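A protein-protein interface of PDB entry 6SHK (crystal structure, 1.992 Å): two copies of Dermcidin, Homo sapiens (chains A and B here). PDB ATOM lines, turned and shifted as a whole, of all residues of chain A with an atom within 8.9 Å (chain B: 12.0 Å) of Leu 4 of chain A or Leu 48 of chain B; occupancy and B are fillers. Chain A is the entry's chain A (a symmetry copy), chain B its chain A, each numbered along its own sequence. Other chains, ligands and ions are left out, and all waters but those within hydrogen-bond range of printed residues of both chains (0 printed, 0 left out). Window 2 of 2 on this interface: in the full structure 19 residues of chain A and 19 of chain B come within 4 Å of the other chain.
The side-chain hydroxyl (OG) of Ser 2 of chain A lies within hydrogen-bond range of the backbone NH (N) of Leu 4 of chain A (2.9 Å). The backbone NH of Glu 5 of chain A is in hydrogen-bond range of the side-chain hydroxyl of Ser 2 of chain A (3.4 Å).
No position is printed for both chains. Of the 7 pairs that touch across the chains among the printed residues, none has its exchanged pair printed and touching as well.
Among the printed residues, pairs that only touch across the chains: Glu 5 of chain A with Lys 41 of chain B (3.2 Å), Leu 8 of chain A with Val 40 of chain B (3.5 Å), Leu 4 of chain A with Leu 48 of chain B (3.5 Å), Leu 4 of chain A with Leu 44 of chain B (3.5 Å), Leu 8 of chain A with Val 37 of chain B (3.5 Å), Leu 8 of chain A with Lys 41 of chain B (3.6 Å) and Ala 11 of chain A with Val 37 of chain B (3.9 Å).
No residue of chain B comes within 4 Å of Ser 2 of chain A. No residue of chain B comes within 4 Å of Leu 3 of chain A. Leu 4 of chain A touches two residues of chain B. Glu 5 of chain A touches one residue of chain B. No residue of chain B comes within 4 Å of Gly 7 of chain A. Of chain B, only Val 37 (3.5 Å), Val 40 (3.5 Å) and Lys 41 (3.6 Å) come within 4 Å of Leu 8 of chain A. Printed residues of chain B within 4 Å of Ala 11 of chain A: Val 37 (3.9 Å). Of the printed residues of chain A, Val 37 of chain B touches Leu 8 and Ala 11. Printed residues of chain A within 4 Å of Val 40 of chain B: Leu 8 (3.5 Å). Of the printed residues of chain A, Lys 41 of chain B touches Glu 5 (3.2 Å) and Leu 8 (3.6 Å). Of the printed residues of chain A, Leu 44 of chain B touches Leu 4. No residue of chain A comes within 4 Å of Val 47 of chain B. Of the printed residues of chain A, Leu 48 of chain B touches Leu 4 (3.5 Å). The nearest residue of chain A that does not touch Leu 48 of chain B is Ser 2 of chain A (5.1 Å). The nearest printed residue of chain A that does not touch Val 37 of chain B is Asp 9 of chain A (5.2 Å).
Of the 13 printed residues of chain B, 5 touch a printed residue of chain A. Printed residues of chain B that touch a printed residue of chain A: Val 37, Val 40, Lys 41, Leu 44 and Leu 48. Hydrophobic or aromatic side chains of chain B within 4 Å of the printed part of chain A: Val 37, Val 40, Leu 44 and Leu 48. Of the 11 printed residues of chain A, 4 touch a printed residue of chain B. Printed residues of chain A that touch a printed residue of chain B: Leu 4, Glu 5, Leu 8 and Ala 11. Hydrophobic or aromatic side chains of chain A within 4 Å of the printed part of chain B: Leu 4, Leu 8 and Ala 11. Among the printed residues, 7 pairs touch across the chains.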
ATOM      1  N   SER A   1      19.421 -15.927 -22.559  1.00  0.00           N
ATOM      2  CA  SER A   1      19.453 -17.069 -21.650  1.00  0.00           C
ATOM      3  C   SER A   1      18.765 -16.718 -20.328  1.00  0.00           C
ATOM      4  O   SER A   1      18.636 -15.545 -19.979  1.00  0.00           O
ATOM      5  CB  SER A   1      20.894 -17.537 -21.400  1.00  0.00           C
ATOM      6  OG  SER A   1      21.539 -16.787 -20.378  1.00  0.00           O
ATOM      7  N   SER A   2      18.352 -17.744 -19.587  1.00  0.00           N
ATOM      8  CA  SER A   2      17.443 -17.550 -18.463  1.00  0.00           C
ATOM      9  C   SER A   2      18.153 -16.958 -17.250  1.00  0.00           C
ATOM     10  O   SER A   2      19.204 -17.450 -16.825  1.00  0.00           O
ATOM     11  CB  SER A   2      16.792 -18.881 -18.084  1.00  0.00           C
ATOM     12  OG  SER A   2      16.219 -18.827 -16.789  1.00  0.00           O
ATOM     13  N   LEU A   3      17.557 -15.908 -16.674  1.00  0.00           N
ATOM     14  CA  LEU A   3      18.044 -15.394 -15.398  1.00  0.00           C
ATOM     15  C   LEU A   3      17.931 -16.442 -14.303  1.00  0.00           C
ATOM     16  O   LEU A   3      18.764 -16.472 -13.390  1.00  0.00           O
ATOM     17  CB  LEU A   3      17.262 -14.145 -14.984  1.00  0.00           C
ATOM     18  CG  LEU A   3      17.518 -12.777 -15.626  1.00  0.00           C
ATOM     19  CD1 LEU A   3      17.144 -12.734 -17.113  1.00  0.00           C
ATOM     20  CD2 LEU A   3      16.763 -11.704 -14.845  1.00  0.00           C
ATOM     21  N   LEU A   4      16.905 -17.298 -14.380  1.00  0.00           N
ATOM     22  CA  LEU A   4      16.568 -18.276 -13.349  1.00  0.00           C
ATOM     23  C   LEU A   4      17.664 -19.310 -13.115  1.00  0.00           C
ATOM     24  O   LEU A   4      18.141 -19.467 -11.987  1.00  0.00           O
ATOM     25  CB  LEU A   4      15.274 -18.999 -13.710  1.00  0.00           C
ATOM     26  CG  LEU A   4      13.998 -18.628 -12.972  1.00  0.00           C
ATOM     27  CD1 LEU A   4      12.808 -19.329 -13.619  1.00  0.00           C
ATOM     28  CD2 LEU A   4      14.130 -19.016 -11.515  1.00  0.00           C
ATOM     29  N   GLU A   5      18.034 -20.068 -14.154  1.00  0.00           N
ATOM     30  CA  GLU A   5      19.131 -21.011 -13.980  1.00  0.00           C
ATOM     31  C   GLU A   5      20.426 -20.269 -13.708  1.00  0.00           C
ATOM     32  O   GLU A   5      21.291 -20.774 -12.987  1.00  0.00           O
ATOM     33  CB  GLU A   5      19.274 -21.926 -15.200  1.00  0.00           C
ATOM     34  CG  GLU A   5      19.493 -23.414 -14.856  1.00  0.00           C
ATOM     35  CD  GLU A   5      20.954 -23.792 -14.652  1.00  0.00           C
ATOM     36  OE1 GLU A   5      21.273 -25.001 -14.652  1.00  0.00           O
ATOM     37  OE2 GLU A   5      21.788 -22.882 -14.501  1.00  0.00           O
ATOM     38  N   LYS A   6      20.571 -19.069 -14.272  1.00  0.00           N
ATOM     39  CA  LYS A   6      21.706 -18.232 -13.921  1.00  0.00           C
ATOM     40  C   LYS A   6      21.738 -17.962 -12.428  1.00  0.00           C
ATOM     41  O   LYS A   6      22.807 -17.994 -11.811  1.00  0.00           O
ATOM     42  CB  LYS A   6      21.654 -16.925 -14.715  1.00  0.00           C
ATOM     43  CG  LYS A   6      22.702 -15.899 -14.303  1.00  0.00           C
ATOM     44  CD  LYS A   6      22.923 -14.871 -15.404  1.00  0.00           C
ATOM     45  CE  LYS A   6      23.602 -15.505 -16.613  1.00  0.00           C
ATOM     46  NZ  LYS A   6      23.897 -14.524 -17.697  1.00  0.00           N
ATOM     47  N   GLY A   7      20.577 -17.729 -11.821  1.00  0.00           N
ATOM     48  CA  GLY A   7      20.558 -17.469 -10.393  1.00  0.00           C
ATOM     49  C   GLY A   7      20.892 -18.702  -9.578  1.00  0.00           C
ATOM     50  O   GLY A   7      21.629 -18.631  -8.591  1.00  0.00           O
ATOM     51  N   LEU A   8      20.339 -19.852  -9.962  1.00  0.00           N
ATOM     52  CA  LEU A   8      20.655 -21.066  -9.214  1.00  0.00           C
ATOM     53  C   LEU A   8      22.136 -21.402  -9.316  1.00  0.00           C
ATOM     54  O   LEU A   8      22.716 -21.975  -8.384  1.00  0.00           O
ATOM     55  CB  LEU A   8      19.803 -22.224  -9.713  1.00  0.00           C
ATOM     56  CG  LEU A   8      18.304 -21.924  -9.705  1.00  0.00           C
ATOM     57  CD1 LEU A   8      17.553 -23.146 -10.154  1.00  0.00           C
ATOM     58  CD2 LEU A   8      17.840 -21.471  -8.325  1.00  0.00           C
ATOM     59  N   ASP A   9      22.760 -21.077 -10.454  1.00  0.00           N
ATOM     60  CA  ASP A   9      24.207 -21.237 -10.580  1.00  0.00           C
ATOM     61  C   ASP A   9      24.937 -20.282  -9.645  1.00  0.00           C
ATOM     62  O   ASP A   9      25.934 -20.653  -9.014  1.00  0.00           O
ATOM     63  CB  ASP A   9      24.639 -21.017 -12.033  1.00  0.00           C
ATOM     64  CG  ASP A   9      24.224 -22.160 -12.962  1.00  0.00           C
ATOM     65  OD1 ASP A   9      23.800 -23.225 -12.460  1.00  0.00           O
ATOM     66  OD2 ASP A   9      24.317 -21.983 -14.204  1.00  0.00           O
ATOM     67  N   GLY A  10      24.453 -19.042  -9.547  1.00  0.00           N
ATOM     68  CA  GLY A  10      24.962 -18.145  -8.524  1.00  0.00           C
ATOM     69  C   GLY A  10      24.940 -18.781  -7.148  1.00  0.00           C
ATOM     70  O   GLY A  10      25.939 -18.761  -6.425  1.00  0.00           O
ATOM     71  N   ALA A  11      23.803 -19.376  -6.777  1.00  0.00           N
ATOM     72  CA  ALA A  11      23.702 -20.057  -5.491  1.00  0.00           C
ATOM     73  C   ALA A  11      24.682 -21.221  -5.411  1.00  0.00           C
ATOM     74  O   ALA A  11      25.436 -21.347  -4.435  1.00  0.00           O
ATOM     75  CB  ALA A  11      22.272 -20.543  -5.266  1.00  0.00           C
ATOM     76  N   ALA B  36      20.147 -29.058  -2.608  1.00  0.00           N
ATOM     77  CA  ALA B  36      18.982 -28.186  -2.643  1.00  0.00           C
ATOM     78  C   ALA B  36      18.890 -27.454  -3.974  1.00  0.00           C
ATOM     79  O   ALA B  36      17.826 -27.419  -4.603  1.00  0.00           O
ATOM     80  CB  ALA B  36      19.035 -27.201  -1.475  1.00  0.00           C
ATOM     81  N   VAL B  37      20.005 -26.889  -4.441  1.00  0.00           N
ATOM     82  CA  VAL B  37      19.987 -26.210  -5.735  1.00  0.00           C
ATOM     83  C   VAL B  37      19.591 -27.180  -6.838  1.00  0.00           C
ATOM     84  O   VAL B  37      18.831 -26.828  -7.747  1.00  0.00           O
ATOM     85  CB  VAL B  37      21.346 -25.569  -6.033  1.00  0.00           C
ATOM     86  CG1 VAL B  37      21.389 -25.124  -7.472  1.00  0.00           C
ATOM     87  CG2 VAL B  37      21.599 -24.390  -5.104  1.00  0.00           C
ATOM     88  N   HIS B  38      20.128 -28.406  -6.799  1.00  0.00           N
ATOM     89  CA  HIS B  38      19.751 -29.365  -7.830  1.00  0.00           C
ATOM     90  C   HIS B  38      18.260 -29.671  -7.781  1.00  0.00           C
ATOM     91  O   HIS B  38      17.584 -29.635  -8.814  1.00  0.00           O
ATOM     92  CB  HIS B  38      20.540 -30.656  -7.709  1.00  0.00           C
ATOM     93  CG  HIS B  38      20.064 -31.726  -8.645  1.00  0.00           C
ATOM     94  ND1 HIS B  38      20.283 -31.678 -10.004  1.00  0.00           N
ATOM     95  CD2 HIS B  38      19.344 -32.852  -8.422  1.00  0.00           C
ATOM     96  CE1 HIS B  38      19.741 -32.739 -10.575  1.00  0.00           C
ATOM     97  NE2 HIS B  38      19.163 -33.467  -9.639  1.00  0.00           N
ATOM     98  N   ASP B  39      17.739 -30.009  -6.597  1.00  0.00           N
ATOM     99  CA  ASP B  39      16.318 -30.301  -6.475  1.00  0.00           C
ATOM    100  C   ASP B  39      15.465 -29.121  -6.922  1.00  0.00           C
ATOM    101  O   ASP B  39      14.366 -29.321  -7.460  1.00  0.00           O
ATOM    102  CB  ASP B  39      15.991 -30.705  -5.042  1.00  0.00           C
ATOM    103  CG  ASP B  39      16.688 -32.002  -4.627  1.00  0.00           C
ATOM    104  OD1 ASP B  39      17.065 -32.798  -5.515  1.00  0.00           O
ATOM    105  OD2 ASP B  39      16.863 -32.226  -3.408  1.00  0.00           O
ATOM    106  N   VAL B  40      15.951 -27.889  -6.735  1.00  0.00           N
ATOM    107  CA  VAL B  40      15.192 -26.746  -7.225  1.00  0.00           C
ATOM    108  C   VAL B  40      15.184 -26.727  -8.747  1.00  0.00           C
ATOM    109  O   VAL B  40      14.121 -26.608  -9.368  1.00  0.00           O
ATOM    110  CB  VAL B  40      15.737 -25.436  -6.645  1.00  0.00           C
ATOM    111  CG1 VAL B  40      15.485 -24.315  -7.607  1.00  0.00           C
ATOM    112  CG2 VAL B  40      15.011 -25.131  -5.370  1.00  0.00           C
ATOM    113  N   LYS B  41      16.365 -26.869  -9.368  1.00  0.00           N
ATOM    114  CA  LYS B  41      16.435 -26.992 -10.814  1.00  0.00           C
ATOM    115  C   LYS B  41      15.454 -28.031 -11.342  1.00  0.00           C
ATOM    116  O   LYS B  41      14.866 -27.832 -12.410  1.00  0.00           O
ATOM    117  CB  LYS B  41      17.831 -27.373 -11.287  1.00  0.00           C
ATOM    118  CG  LYS B  41      18.882 -26.260 -11.275  1.00  0.00           C
ATOM    119  CD  LYS B  41      20.147 -26.639 -12.092  1.00  0.00           C
ATOM    120  CE  LYS B  41      21.093 -27.604 -11.338  1.00  0.00           C
ATOM    121  NZ  LYS B  41      22.302 -28.054 -12.123  1.00  0.00           N
ATOM    122  N   ASP B  42      15.282 -29.150 -10.624  1.00  0.00           N
ATOM    123  CA  ASP B  42      14.357 -30.174 -11.084  1.00  0.00           C
ATOM    124  C   ASP B  42      12.940 -29.617 -11.206  1.00  0.00           C
ATOM    125  O   ASP B  42      12.273 -29.848 -12.216  1.00  0.00           O
ATOM    126  CB  ASP B  42      14.381 -31.397 -10.168  1.00  0.00           C
ATOM    127  CG  ASP B  42      15.671 -32.234 -10.315  1.00  0.00           C
ATOM    128  OD1 ASP B  42      16.289 -32.220 -11.406  1.00  0.00           O
ATOM    129  OD2 ASP B  42      16.059 -32.911  -9.339  1.00  0.00           O
ATOM    130  N   VAL B  43      12.479 -28.847 -10.212  1.00  0.00           N
ATOM    131  CA  VAL B  43      11.112 -28.327 -10.281  1.00  0.00           C
ATOM    132  C   VAL B  43      10.948 -27.347 -11.436  1.00  0.00           C
ATOM    133  O   VAL B  43       9.872 -27.267 -12.045  1.00  0.00           O
ATOM    134  CB  VAL B  43      10.695 -27.683  -8.949  1.00  0.00           C
ATOM    135  CG1 VAL B  43       9.181 -27.394  -8.955  1.00  0.00           C
ATOM    136  CG2 VAL B  43      11.062 -28.593  -7.796  1.00  0.00           C
ATOM    137  N   LEU B  44      11.996 -26.603 -11.762  1.00  0.00           N
ATOM    138  CA  LEU B  44      11.998 -25.670 -12.877  1.00  0.00           C
ATOM    139  C   LEU B  44      12.422 -26.323 -14.187  1.00  0.00           C
ATOM    140  O   LEU B  44      12.600 -25.621 -15.189  1.00  0.00           O
ATOM    141  CB  LEU B  44      12.922 -24.491 -12.574  1.00  0.00           C
ATOM    142  CG  LEU B  44      12.450 -23.328 -11.698  1.00  0.00           C
ATOM    143  CD1 LEU B  44      11.755 -23.764 -10.409  1.00  0.00           C
ATOM    144  CD2 LEU B  44      13.663 -22.497 -11.383  1.00  0.00           C
ATOM    145  N   ASP B  45      12.629 -27.636 -14.188  1.00  0.00           N
ATOM    146  CA  ASP B  45      12.720 -28.428 -15.407  1.00  0.00           C
ATOM    147  C   ASP B  45      11.371 -29.021 -15.790  1.00  0.00           C
ATOM    148  O   ASP B  45      10.973 -28.948 -16.958  1.00  0.00           O
ATOM    149  CB  ASP B  45      13.758 -29.549 -15.239  1.00  0.00           C
ATOM    150  CG  ASP B  45      14.296 -30.076 -16.573  1.00  0.00           C
ATOM    151  OD1 ASP B  45      13.514 -30.215 -17.548  1.00  0.00           O
ATOM    152  OD2 ASP B  45      15.512 -30.363 -16.639  1.00  0.00           O
ATOM    153  N   SER B  46      10.640 -29.576 -14.822  1.00  0.00           N
ATOM    154  CA  SER B  46       9.320 -30.141 -15.081  1.00  0.00           C
ATOM    155  C   SER B  46       8.234 -29.079 -15.213  1.00  0.00           C
ATOM    156  O   SER B  46       7.047 -29.424 -15.281  1.00  0.00           O
ATOM    157  CB  SER B  46       8.942 -31.128 -13.972  1.00  0.00           C
ATOM    158  OG  SER B  46       8.785 -30.462 -12.729  1.00  0.00           O
ATOM    159  N   VAL B  47       8.607 -27.803 -15.248  1.00  0.00           N
ATOM    160  CA  VAL B  47       7.628 -26.729 -15.334  1.00  0.00           C
ATOM    161  C   VAL B  47       8.095 -25.698 -16.358  1.00  0.00           C
ATOM    162  O   VAL B  47       7.292 -25.181 -17.146  1.00  0.00           O
ATOM    163  CB  VAL B  47       7.380 -26.103 -13.949  1.00  0.00           C
ATOM    164  CG1 VAL B  47       6.806 -24.701 -14.081  1.00  0.00           C
ATOM    165  CG2 VAL B  47       6.430 -26.981 -13.143  1.00  0.00           C
ATOM    166  N   LEU B  48       9.389 -25.407 -16.373  1.00  0.00           N
ATOM    167  CA  LEU B  48       9.922 -24.465 -17.350  1.00  0.00           C
ATOM    168  C   LEU B  48      11.302 -24.889 -17.837  1.00  0.00           C
ATOM    169  O   LEU B  48      11.432 -25.495 -18.902  1.00  0.00           O
ATOM    170  CB  LEU B  48       9.972 -23.051 -16.763  1.00  0.00           C
ATOM    171  CG  LEU B  48      11.121 -22.637 -15.843  1.00  0.00           C
ATOM    172  CD1 LEU B  48      12.173 -21.861 -16.627  1.00  0.00           C
ATOM    173  CD2 LEU B  48      10.573 -21.811 -14.697  1.00  0.00           C
